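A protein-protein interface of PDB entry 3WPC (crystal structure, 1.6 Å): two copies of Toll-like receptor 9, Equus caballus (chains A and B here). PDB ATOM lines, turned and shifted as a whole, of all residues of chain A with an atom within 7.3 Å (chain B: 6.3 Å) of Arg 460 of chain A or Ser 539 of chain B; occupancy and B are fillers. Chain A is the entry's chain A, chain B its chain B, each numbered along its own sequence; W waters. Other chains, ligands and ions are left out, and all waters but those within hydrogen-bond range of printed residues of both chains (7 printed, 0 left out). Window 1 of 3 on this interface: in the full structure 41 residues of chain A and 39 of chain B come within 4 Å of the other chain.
Printed residues of chain B within 4 Å of Arg 460 of chain A: Gln 536 and Ser 539.
Of the printed residues of chain A, Ser 539 of chain B touches Arg 460.
Printed residues of chain A within 4 Å of Gln 536 of chain B: Arg 460 (3.5 Å) and His 484 (3.6 Å).
Of the printed residues of chain B, Asp 403 of chain A touches Met 540.
Of the printed residues of chain B, Met 379 of chain A touches Met 540 (3.7 Å) and Arg 541 (3.2 Å).
Ser 459 of chain A touches none of the printed residues of chain B.
The backbone NH (N) of Arg 460 of chain A is in hydrogen-bond range of the backbone carbonyl oxygen (O) of Ser 483 of chain A, 2.9 Å away.
O of Arg 460 of chain A lies within hydrogen-bond range of N of Asp 403 of chain A, 3.1 Å away.
The backbone NH (N) of Asn 462 of chain A lies within hydrogen-bond range of the side-chain amide oxygen (OD1) of Asn 485 of chain A (3.4 Å).
OG of Ser 539 of chain B sits at hydrogen-bond distance from O of Ser 535 of chain B, 3.0 Å away.
The backbone NH of His 484 of chain A lies close to the backbone carbonyl oxygen of His 509 of chain A (3.3 Å).
The backbone carbonyl oxygen (O) of Leu 482 of chain A is in hydrogen-bond range of the side-chain amide nitrogen (ND2) of Asn 485 of chain A (3.1 Å).
SD of Met 379 of chain A sits close to O of Arg 541 of chain B (3.2 Å).
NZ of Lys 511 of chain B is in hydrogen-bond range of O of Asn 485 of chain A (3.0 Å).
O of His 484 of chain A lies within hydrogen-bond range of NZ of Lys 511 of chain B.
No position is printed for both chains.
Hydrophobic or aromatic side chains of chain B within 4 Å of the printed part of chain A: Met 540.
Hydrophobic or aromatic side chains of chain A within 4 Å of the printed part of chain B: Met 379 and His 484.
CG of Met 379 of chain A touches CG of Met 540 of chain B, 3.7 Å away.
OD1 of Asp 403 of chain A touches CE of Met 540 of chain B (3.5 Å).
CB of Arg 460 of chain A touches NE2 of Gln 536 of chain B, at 3.5 Å.
Ser 539 of chain B touches Arg 460 of chain A.
OE1 of Gln 536 of chain B touches O of His 484 of chain A, 3.6 Å away.
Water W2 lies within hydrogen-bond range of O of Asn 461 of chain A, NE2 of Gln 536 of chain B, NZ of Lys 511 of chain B and O of His 484 of chain A.
Water W7 lies within hydrogen-bond range of the side-chain carboxylate of Asp 403 of chain A (2.7 Å) and the side-chain amide nitrogen of Gln 536 of chain B (3.0 Å).
Water W4 lies within hydrogen-bond range of the side-chain carboxylate (OD1) of Asp 403 of chain A, the backbone carbonyl oxygen (O) of Gln 536 of chain B and the guanidinium group (NH1) of Arg 460 of chain A.
Water W6 lies within hydrogen-bond range of the backbone carbonyl oxygen (O) of Arg 541 of chain B (2.8 Å) and the side-chain sulfur (SD) of Met 379 of chain A (3.7 Å).
Water W3 lies within hydrogen-bond range of O of His 509 of chain A (2.9 Å), NZ of Lys 511 of chain B (3.1 Å) and O of Asn 485 of chain A (3.3 Å).
Water W1 lies within hydrogen-bond range of the guanidinium group of Arg 460 of chain A (3.0 Å) and the side-chain hydroxyl of Ser 539 of chain B (3.3 Å).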
ATOM      1  N   MET A 379      34.252   3.113   4.580  1.00  0.00           N
ATOM      2  CA  MET A 379      34.689   2.212   5.644  1.00  0.00           C
ATOM      3  C   MET A 379      36.132   2.324   5.977  1.00  0.00           C
ATOM      4  O   MET A 379      36.829   1.296   6.113  1.00  0.00           O
ATOM      5  CB  MET A 379      34.364   0.777   5.322  1.00  0.00           C
ATOM      6  CG  MET A 379      32.946   0.556   4.964  1.00  0.00           C
ATOM      7  SD  MET A 379      32.565  -1.177   4.752  1.00  0.00           S
ATOM      8  CE  MET A 379      30.882  -1.021   4.221  1.00  0.00           C
ATOM      9  N   LEU A 401      32.463   8.081  -0.043  1.00  0.00           N
ATOM     10  CA  LEU A 401      33.109   8.302   1.255  1.00  0.00           C
ATOM     11  C   LEU A 401      32.208   7.953   2.430  1.00  0.00           C
ATOM     12  O   LEU A 401      32.438   8.412   3.590  1.00  0.00           O
ATOM     13  CB  LEU A 401      33.662   9.707   1.357  1.00  0.00           C
ATOM     14  CG  LEU A 401      35.064   9.928   0.792  1.00  0.00           C
ATOM     15  CD1 LEU A 401      35.409  11.377   0.581  1.00  0.00           C
ATOM     16  CD2 LEU A 401      36.066   9.353   1.801  1.00  0.00           C
ATOM     17  N   SER A 402      31.304   7.043   2.167  1.00  0.00           N
ATOM     18  CA  SER A 402      30.337   6.632   3.214  1.00  0.00           C
ATOM     19  C   SER A 402      31.002   5.857   4.330  1.00  0.00           C
ATOM     20  O   SER A 402      32.068   5.291   4.141  1.00  0.00           O
ATOM     21  CB  SER A 402      29.135   5.883   2.654  1.00  0.00           C
ATOM     22  OG  SER A 402      29.434   4.669   2.035  1.00  0.00           O
ATOM     23  N   ASP A 403      30.308   5.735   5.452  1.00  0.00           N
ATOM     24  CA  ASP A 403      30.834   4.878   6.541  1.00  0.00           C
ATOM     25  C   ASP A 403      32.252   5.322   6.978  1.00  0.00           C
ATOM     26  O   ASP A 403      33.210   4.518   7.129  1.00  0.00           O
ATOM     27  CB  ASP A 403      30.743   3.387   6.208  1.00  0.00           C
ATOM     28  CG  ASP A 403      29.393   2.807   6.349  1.00  0.00           C
ATOM     29  OD1 ASP A 403      28.761   2.910   7.449  1.00  0.00           O
ATOM     30  OD2 ASP A 403      28.957   2.105   5.447  1.00  0.00           O
ATOM     31  N   ASN A 404      32.397   6.616   7.206  1.00  0.00           N
ATOM     32  CA  ASN A 404      33.595   7.232   7.745  1.00  0.00           C
ATOM     33  C   ASN A 404      33.208   8.090   8.952  1.00  0.00           C
ATOM     34  O   ASN A 404      32.037   8.035   9.410  1.00  0.00           O
ATOM     35  CB  ASN A 404      34.345   7.994   6.647  1.00  0.00           C
ATOM     36  CG  ASN A 404      35.134   7.056   5.764  1.00  0.00           C
ATOM     37  OD1 ASN A 404      36.007   6.365   6.265  1.00  0.00           O
ATOM     38  ND2 ASN A 404      34.838   7.010   4.495  1.00  0.00           N
ATOM     39  N   ARG A 405      34.157   8.875   9.464  1.00  0.00           N
ATOM     40  CA  ARG A 405      33.944   9.687  10.669  1.00  0.00           C
ATOM     41  C   ARG A 405      34.185  11.190  10.396  1.00  0.00           C
ATOM     42  O   ARG A 405      34.605  11.948  11.247  1.00  0.00           O
ATOM     43  CB  ARG A 405      34.810   9.158  11.800  1.00  0.00           C
ATOM     44  CG  ARG A 405      34.533   7.708  12.115  1.00  0.00           C
ATOM     45  CD  ARG A 405      35.365   7.199  13.275  1.00  0.00           C
ATOM     46  NE  ARG A 405      36.773   7.344  12.931  1.00  0.00           N
ATOM     47  CZ  ARG A 405      37.787   6.776  13.577  1.00  0.00           C
ATOM     48  NH1 ARG A 405      37.579   5.966  14.637  1.00  0.00           N
ATOM     49  NH2 ARG A 405      39.017   7.015  13.128  1.00  0.00           N
ATOM     50  N   ILE A 406      33.841  11.611   9.180  1.00  0.00           N
ATOM     51  CA  ILE A 406      34.004  12.991   8.772  1.00  0.00           C
ATOM     52  C   ILE A 406      32.925  13.813   9.467  1.00  0.00           C
ATOM     53  O   ILE A 406      31.786  13.364   9.567  1.00  0.00           O
ATOM     54  CB  ILE A 406      33.954  13.092   7.256  1.00  0.00           C
ATOM     55  CG1 ILE A 406      35.135  12.345   6.678  1.00  0.00           C
ATOM     56  CG2 ILE A 406      33.939  14.520   6.789  1.00  0.00           C
ATOM     57  CD1 ILE A 406      35.009  11.990   5.226  1.00  0.00           C
ATOM     58  N   ASP A 457      29.064  10.500  -2.184  1.00  0.00           N
ATOM     59  CA  ASP A 457      28.386   9.828  -1.065  1.00  0.00           C
ATOM     60  C   ASP A 457      29.130  10.049   0.226  1.00  0.00           C
ATOM     61  O   ASP A 457      30.172   9.484   0.465  1.00  0.00           O
ATOM     62  CB  ASP A 457      28.129   8.373  -1.392  1.00  0.00           C
ATOM     63  CG  ASP A 457      27.094   7.727  -0.479  1.00  0.00           C
ATOM     64  OD1 ASP A 457      26.934   8.219   0.641  1.00  0.00           O
ATOM     65  OD2 ASP A 457      26.450   6.720  -0.864  1.00  0.00           O
ATOM     66  N   LEU A 458      28.530  10.883   1.085  1.00  0.00           N
ATOM     67  CA  LEU A 458      29.007  11.162   2.452  1.00  0.00           C
ATOM     68  C   LEU A 458      28.005  10.646   3.497  1.00  0.00           C
ATOM     69  O   LEU A 458      27.989  11.091   4.638  1.00  0.00           O
ATOM     70  CB  LEU A 458      29.269  12.644   2.637  1.00  0.00           C
ATOM     71  CG  LEU A 458      30.559  13.214   2.107  1.00  0.00           C
ATOM     72  CD1 LEU A 458      30.542  14.715   2.304  1.00  0.00           C
ATOM     73  CD2 LEU A 458      31.765  12.632   2.853  1.00  0.00           C
ATOM     74  N   SER A 459      27.215   9.645   3.121  1.00  0.00           N
ATOM     75  CA  SER A 459      26.256   9.046   4.044  1.00  0.00           C
ATOM     76  C   SER A 459      26.988   8.258   5.115  1.00  0.00           C
ATOM     77  O   SER A 459      28.066   7.760   4.885  1.00  0.00           O
ATOM     78  CB  SER A 459      25.286   8.098   3.328  1.00  0.00           C
ATOM     79  OG  SER A 459      25.968   6.987   2.746  1.00  0.00           O
ATOM     80  N   ARG A 460      26.365   8.113   6.273  1.00  0.00           N
ATOM     81  CA  ARG A 460      26.956   7.339   7.344  1.00  0.00           C
ATOM     82  C   ARG A 460      28.298   7.930   7.814  1.00  0.00           C
ATOM     83  O   ARG A 460      29.295   7.212   8.036  1.00  0.00           O
ATOM     84  CB  ARG A 460      27.021   5.862   6.972  1.00  0.00           C
ATOM     85  CG  ARG A 460      25.684   5.286   6.563  1.00  0.00           C
ATOM     86  CD  ARG A 460      25.798   3.866   6.065  1.00  0.00           C
ATOM     87  NE  ARG A 460      24.481   3.512   5.541  1.00  0.00           N
ATOM     88  CZ  ARG A 460      23.612   2.717   6.125  1.00  0.00           C
ATOM     89  NH1 ARG A 460      23.948   2.033   7.199  1.00  0.00           N
ATOM     90  NH2 ARG A 460      22.417   2.537   5.574  1.00  0.00           N
ATOM     91  N   ASN A 461      28.308   9.230   7.994  1.00  0.00           N
ATOM     92  CA  ASN A 461      29.381   9.969   8.560  1.00  0.00           C
ATOM     93  C   ASN A 461      28.905  10.671   9.823  1.00  0.00           C
ATOM     94  O   ASN A 461      27.798  10.366  10.308  1.00  0.00           O
ATOM     95  CB  ASN A 461      29.994  10.904   7.511  1.00  0.00           C
ATOM     96  CG  ASN A 461      31.059  10.218   6.653  1.00  0.00           C
ATOM     97  OD1 ASN A 461      32.252  10.226   7.013  1.00  0.00           O
ATOM     98  ND2 ASN A 461      30.639   9.568   5.601  1.00  0.00           N
ATOM     99  N   ASN A 462      29.703  11.587  10.355  1.00  0.00           N
ATOM    100  CA  ASN A 462      29.463  12.146  11.672  1.00  0.00           C
ATOM    101  C   ASN A 462      29.161  13.616  11.625  1.00  0.00           C
ATOM    102  O   ASN A 462      29.459  14.356  12.581  1.00  0.00           O
ATOM    103  CB  ASN A 462      30.644  11.894  12.609  1.00  0.00           C
ATOM    104  CG  ASN A 462      30.779  10.442  12.999  1.00  0.00           C
ATOM    105  OD1 ASN A 462      29.875   9.658  12.794  1.00  0.00           O
ATOM    106  ND2 ASN A 462      31.919  10.094  13.596  1.00  0.00           N
ATOM    107  N   LEU A 463      28.544  14.083  10.535  1.00  0.00           N
ATOM    108  CA  LEU A 463      28.147  15.490  10.500  1.00  0.00           C
ATOM    109  C   LEU A 463      26.992  15.752  11.486  1.00  0.00           C
ATOM    110  O   LEU A 463      26.022  15.014  11.495  1.00  0.00           O
ATOM    111  CB  LEU A 463      27.712  15.923   9.095  1.00  0.00           C
ATOM    112  CG  LEU A 463      28.799  16.363   8.142  1.00  0.00           C
ATOM    113  CD1 LEU A 463      29.489  15.168   7.559  1.00  0.00           C
ATOM    114  CD2 LEU A 463      28.185  17.277   7.061  1.00  0.00           C
ATOM    115  N   ARG A 481      24.921  12.835  -1.160  1.00  0.00           N
ATOM    116  CA  ARG A 481      24.281  11.990  -0.189  1.00  0.00           C
ATOM    117  C   ARG A 481      24.861  12.246   1.172  1.00  0.00           C
ATOM    118  O   ARG A 481      26.061  12.154   1.403  1.00  0.00           O
ATOM    119  CB  ARG A 481      24.388  10.504  -0.562  1.00  0.00           C
ATOM    120  CG  ARG A 481      23.630  10.185  -1.833  1.00  0.00           C
ATOM    121  CD  ARG A 481      23.258   8.705  -1.876  1.00  0.00           C
ATOM    122  NE  ARG A 481      22.578   8.451  -3.123  1.00  0.00           N
ATOM    123  CZ  ARG A 481      21.284   8.646  -3.344  1.00  0.00           C
ATOM    124  NH1 ARG A 481      20.449   9.059  -2.368  1.00  0.00           N
ATOM    125  NH2 ARG A 481      20.821   8.389  -4.561  1.00  0.00           N
ATOM    126  N   LEU A 482      23.976  12.661   2.065  1.00  0.00           N
ATOM    127  CA  LEU A 482      24.318  12.909   3.448  1.00  0.00           C
ATOM    128  C   LEU A 482      23.388  12.117   4.367  1.00  0.00           C
ATOM    129  O   LEU A 482      23.204  12.516   5.519  1.00  0.00           O
ATOM    130  CB  LEU A 482      24.217  14.399   3.756  1.00  0.00           C
ATOM    131  CG  LEU A 482      25.372  15.243   3.244  1.00  0.00           C
ATOM    132  CD1 LEU A 482      25.045  16.703   3.449  1.00  0.00           C
ATOM    133  CD2 LEU A 482      26.637  14.918   4.033  1.00  0.00           C
ATOM    134  N   SER A 483      22.839  10.998   3.898  1.00  0.00           N
ATOM    135  CA  SER A 483      21.900  10.226   4.726  1.00  0.00           C
ATOM    136  C   SER A 483      22.637   9.655   5.923  1.00  0.00           C
ATOM    137  O   SER A 483      23.861   9.509   5.909  1.00  0.00           O
ATOM    138  CB  SER A 483      21.198   9.093   3.971  1.00  0.00           C
ATOM    139  OG  SER A 483      22.076   8.001   3.674  1.00  0.00           O
ATOM    140  N   HIS A 484      21.887   9.373   6.973  1.00  0.00           N
ATOM    141  CA  HIS A 484      22.473   8.688   8.135  1.00  0.00           C
ATOM    142  C   HIS A 484      23.720   9.377   8.712  1.00  0.00           C
ATOM    143  O   HIS A 484      24.666   8.708   9.124  1.00  0.00           O
ATOM    144  CB  HIS A 484      22.837   7.251   7.766  1.00  0.00           C
ATOM    145  CG  HIS A 484      21.695   6.337   7.474  1.00  0.00           C
ATOM    146  ND1 HIS A 484      21.240   6.081   6.200  1.00  0.00           N
ATOM    147  CD2 HIS A 484      20.934   5.595   8.295  1.00  0.00           C
ATOM    148  CE1 HIS A 484      20.268   5.188   6.248  1.00  0.00           C
ATOM    149  NE2 HIS A 484      20.039   4.897   7.510  1.00  0.00           N
ATOM    150  N   ASN A 485      23.738  10.706   8.809  1.00  0.00           N
ATOM    151  CA  ASN A 485      24.664  11.447   9.576  1.00  0.00           C
ATOM    152  C   ASN A 485      23.896  11.744  10.880  1.00  0.00           C
ATOM    153  O   ASN A 485      23.046  10.921  11.247  1.00  0.00           O
ATOM    154  CB  ASN A 485      25.133  12.689   8.802  1.00  0.00           C
ATOM    155  CG  ASN A 485      26.278  12.372   7.831  1.00  0.00           C
ATOM    156  OD1 ASN A 485      27.423  12.701   8.094  1.00  0.00           O
ATOM    157  ND2 ASN A 485      25.968  11.723   6.763  1.00  0.00           N
ATOM    158  N   HIS A 509      17.347  10.193   7.145  1.00  0.00           N
ATOM    159  CA  HIS A 509      17.946   9.674   8.356  1.00  0.00           C
ATOM    160  C   HIS A 509      18.885  10.670   9.045  1.00  0.00           C
ATOM    161  O   HIS A 509      20.016  10.345   9.474  1.00  0.00           O
ATOM    162  CB  HIS A 509      18.615   8.312   8.090  1.00  0.00           C
ATOM    163  CG  HIS A 509      17.699   7.304   7.485  1.00  0.00           C
ATOM    164  ND1 HIS A 509      16.935   6.456   8.254  1.00  0.00           N
ATOM    165  CD2 HIS A 509      17.433   6.983   6.203  1.00  0.00           C
ATOM    166  CE1 HIS A 509      16.258   5.644   7.464  1.00  0.00           C
ATOM    167  NE2 HIS A 509      16.542   5.943   6.218  1.00  0.00           N
ATOM    168  N   LYS B 511      24.680   4.994  17.746  1.00  0.00           N
ATOM    169  CA  LYS B 511      25.547   4.363  16.747  1.00  0.00           C
ATOM    170  C   LYS B 511      26.789   3.812  17.403  1.00  0.00           C
ATOM    171  O   LYS B 511      27.891   3.980  16.903  1.00  0.00           O
ATOM    172  CB  LYS B 511      25.904   5.374  15.651  1.00  0.00           C
ATOM    173  CG  LYS B 511      24.705   6.139  15.154  1.00  0.00           C
ATOM    174  CD  LYS B 511      25.008   6.879  13.855  1.00  0.00           C
ATOM    175  CE  LYS B 511      23.835   7.707  13.438  1.00  0.00           C
ATOM    176  NZ  LYS B 511      24.096   8.257  12.097  1.00  0.00           N
ATOM    177  N   SER B 535      22.167  -0.066  14.952  1.00  0.00           N
ATOM    178  CA  SER B 535      22.393  -0.947  13.796  1.00  0.00           C
ATOM    179  C   SER B 535      23.420  -0.444  12.837  1.00  0.00           C
ATOM    180  O   SER B 535      23.947  -1.253  12.089  1.00  0.00           O
ATOM    181  CB  SER B 535      21.094  -1.207  13.028  1.00  0.00           C
ATOM    182  OG  SER B 535      20.648   0.049  12.456  1.00  0.00           O
ATOM    183  N   GLN B 536      23.760   0.835  12.843  1.00  0.00           N
ATOM    184  CA  GLN B 536      24.621   1.326  11.732  1.00  0.00           C
ATOM    185  C   GLN B 536      25.952   0.599  11.692  1.00  0.00           C
ATOM    186  O   GLN B 536      26.435   0.215  10.625  1.00  0.00           O
ATOM    187  CB  GLN B 536      24.805   2.828  11.798  1.00  0.00           C
ATOM    188  CG  GLN B 536      25.036   3.436  10.440  1.00  0.00           C
ATOM    189  CD  GLN B 536      25.017   4.938  10.508  1.00  0.00           C
ATOM    190  OE1 GLN B 536      23.967   5.546  10.768  1.00  0.00           O
ATOM    191  NE2 GLN B 536      26.169   5.519  10.359  1.00  0.00           N
ATOM    192  N   PRO B 537      26.611   0.409  12.857  1.00  0.00           N
ATOM    193  CA  PRO B 537      27.931  -0.236  12.748  1.00  0.00           C
ATOM    194  C   PRO B 537      27.845  -1.657  12.246  1.00  0.00           C
ATOM    195  O   PRO B 537      28.721  -2.109  11.460  1.00  0.00           O
ATOM    196  CB  PRO B 537      28.458  -0.190  14.200  1.00  0.00           C
ATOM    197  CG  PRO B 537      27.788   1.040  14.767  1.00  0.00           C
ATOM    198  CD  PRO B 537      26.394   1.008  14.184  1.00  0.00           C
ATOM    199  N   PHE B 538      26.801  -2.362  12.684  1.00  0.00           N
ATOM    200  CA  PHE B 538      26.534  -3.760  12.280  1.00  0.00           C
ATOM    201  C   PHE B 538      26.186  -3.875  10.806  1.00  0.00           C
ATOM    202  O   PHE B 538      26.288  -4.982  10.234  1.00  0.00           O
ATOM    203  CB  PHE B 538      25.440  -4.391  13.107  1.00  0.00           C
ATOM    204  CG  PHE B 538      25.849  -4.679  14.489  1.00  0.00           C
ATOM    205  CD1 PHE B 538      26.827  -5.585  14.728  1.00  0.00           C
ATOM    206  CD2 PHE B 538      25.264  -4.048  15.556  1.00  0.00           C
ATOM    207  CE1 PHE B 538      27.218  -5.916  16.036  1.00  0.00           C
ATOM    208  CE2 PHE B 538      25.645  -4.359  16.873  1.00  0.00           C
ATOM    209  CZ  PHE B 538      26.666  -5.270  17.107  1.00  0.00           C
ATOM    210  N   SER B 539      25.844  -2.749  10.175  1.00  0.00           N
ATOM    211  CA  SER B 539      25.486  -2.710   8.794  1.00  0.00           C
ATOM    212  C   SER B 539      26.689  -2.394   7.896  1.00  0.00           C
ATOM    213  O   SER B 539      26.524  -2.292   6.673  1.00  0.00           O
ATOM    214  CB  SER B 539      24.343  -1.705   8.557  1.00  0.00           C
ATOM    215  OG  SER B 539      23.208  -2.112   9.344  1.00  0.00           O
ATOM    216  N   MET B 540      27.868  -2.282   8.489  1.00  0.00           N
ATOM    217  CA  MET B 540      29.050  -1.922   7.754  1.00  0.00           C
ATOM    218  C   MET B 540      29.676  -3.188   7.228  1.00  0.00           C
ATOM    219  O   MET B 540      30.503  -3.785   7.913  1.00  0.00           O
ATOM    220  CB  MET B 540      29.994  -1.152   8.678  1.00  0.00           C
ATOM    221  CG  MET B 540      30.936  -0.250   7.939  1.00  0.00           C
ATOM    222  SD  MET B 540      32.057   0.530   9.093  1.00  0.00           S
ATOM    223  CE  MET B 540      31.100   1.892   9.781  1.00  0.00           C
ATOM    224  N   ARG B 541      29.273  -3.603   6.020  1.00  0.00           N
ATOM    225  CA  ARG B 541      29.607  -4.895   5.455  1.00  0.00           C
ATOM    226  C   ARG B 541      31.105  -5.078   5.420  1.00  0.00           C
ATOM    227  O   ARG B 541      31.800  -4.288   4.792  1.00  0.00           O
ATOM    228  N   HIS B 545      32.597  -6.929  14.566  1.00  0.00           N
ATOM    229  CA  HIS B 545      32.184  -6.424  15.851  1.00  0.00           C
ATOM    230  C   HIS B 545      32.324  -7.542  16.873  1.00  0.00           C
ATOM    231  O   HIS B 545      32.570  -8.669  16.527  1.00  0.00           O
ATOM    232  CB  HIS B 545      30.784  -5.831  15.762  1.00  0.00           C
ATOM    233  CG  HIS B 545      30.746  -4.670  14.832  1.00  0.00           C
ATOM    234  ND1 HIS B 545      30.546  -4.834  13.482  1.00  0.00           N
ATOM    235  CD2 HIS B 545      31.084  -3.374  15.006  1.00  0.00           C
ATOM    236  CE1 HIS B 545      30.647  -3.666  12.884  1.00  0.00           C
ATOM    237  NE2 HIS B 545      30.996  -2.766  13.779  1.00  0.00           N
ATOM    238  N   ASN B 564      19.284  -4.509  15.783  1.00  0.00           N
ATOM    239  CA  ASN B 564      20.627  -4.131  15.371  1.00  0.00           C
ATOM    240  C   ASN B 564      21.080  -4.692  14.030  1.00  0.00           C
ATOM    241  O   ASN B 564      22.176  -4.386  13.626  1.00  0.00           O
ATOM    242  CB  ASN B 564      21.614  -4.551  16.471  1.00  0.00           C
ATOM    243  CG  ASN B 564      21.692  -3.531  17.568  1.00  0.00           C
ATOM    244  OD1 ASN B 564      21.547  -2.332  17.313  1.00  0.00           O
ATOM    245  ND2 ASN B 564      21.803  -3.986  18.810  1.00  0.00           N
ATOM    246  N   GLY B 565      20.265  -5.523  13.384  1.00  0.00           N
ATOM    247  CA  GLY B 565      20.671  -6.151  12.094  1.00  0.00           C
ATOM    248  C   GLY B 565      21.924  -7.001  12.175  1.00  0.00           C
ATOM    249  O   GLY B 565      22.696  -7.089  11.213  1.00  0.00           O
ATOM    250  N   HIS B 567      24.300  -9.881  11.814  1.00  0.00           N
ATOM    251  CA  HIS B 567      24.121 -10.895  10.808  1.00  0.00           C
ATOM    252  C   HIS B 567      25.414 -11.609  10.414  1.00  0.00           C
ATOM    253  O   HIS B 567      25.370 -12.727   9.876  1.00  0.00           O
ATOM    254  CB  HIS B 567      23.483 -10.309   9.555  1.00  0.00           C
ATOM    255  CG  HIS B 567      24.375  -9.424   8.795  1.00  0.00           C
ATOM    256  ND1 HIS B 567      24.624  -8.119   9.163  1.00  0.00           N
ATOM    257  CD2 HIS B 567      25.081  -9.635   7.651  1.00  0.00           C
ATOM    258  CE1 HIS B 567      25.483  -7.583   8.311  1.00  0.00           C
ATOM    259  NE2 HIS B 567      25.775  -8.482   7.391  1.00  0.00           N
HETATM  260  O   HOH W   1      22.026   0.969   9.267  1.00  0.00           O
HETATM  261  O   HOH W   2      26.888   8.150  11.228  1.00  0.00           O
HETATM  262  O   HOH W   3      21.113   8.203  11.155  1.00  0.00           O
HETATM  263  O   HOH W   4      26.689   1.204   8.061  1.00  0.00           O
HETATM  264  O   HOH W   5      26.936   0.362   5.331  1.00  0.00           O
HETATM  265  O   HOH W   6      32.242  -3.743   2.040  1.00  0.00           O
HETATM  266  O   HOH W   7      28.765   4.162   9.877  1.00  0.00           O
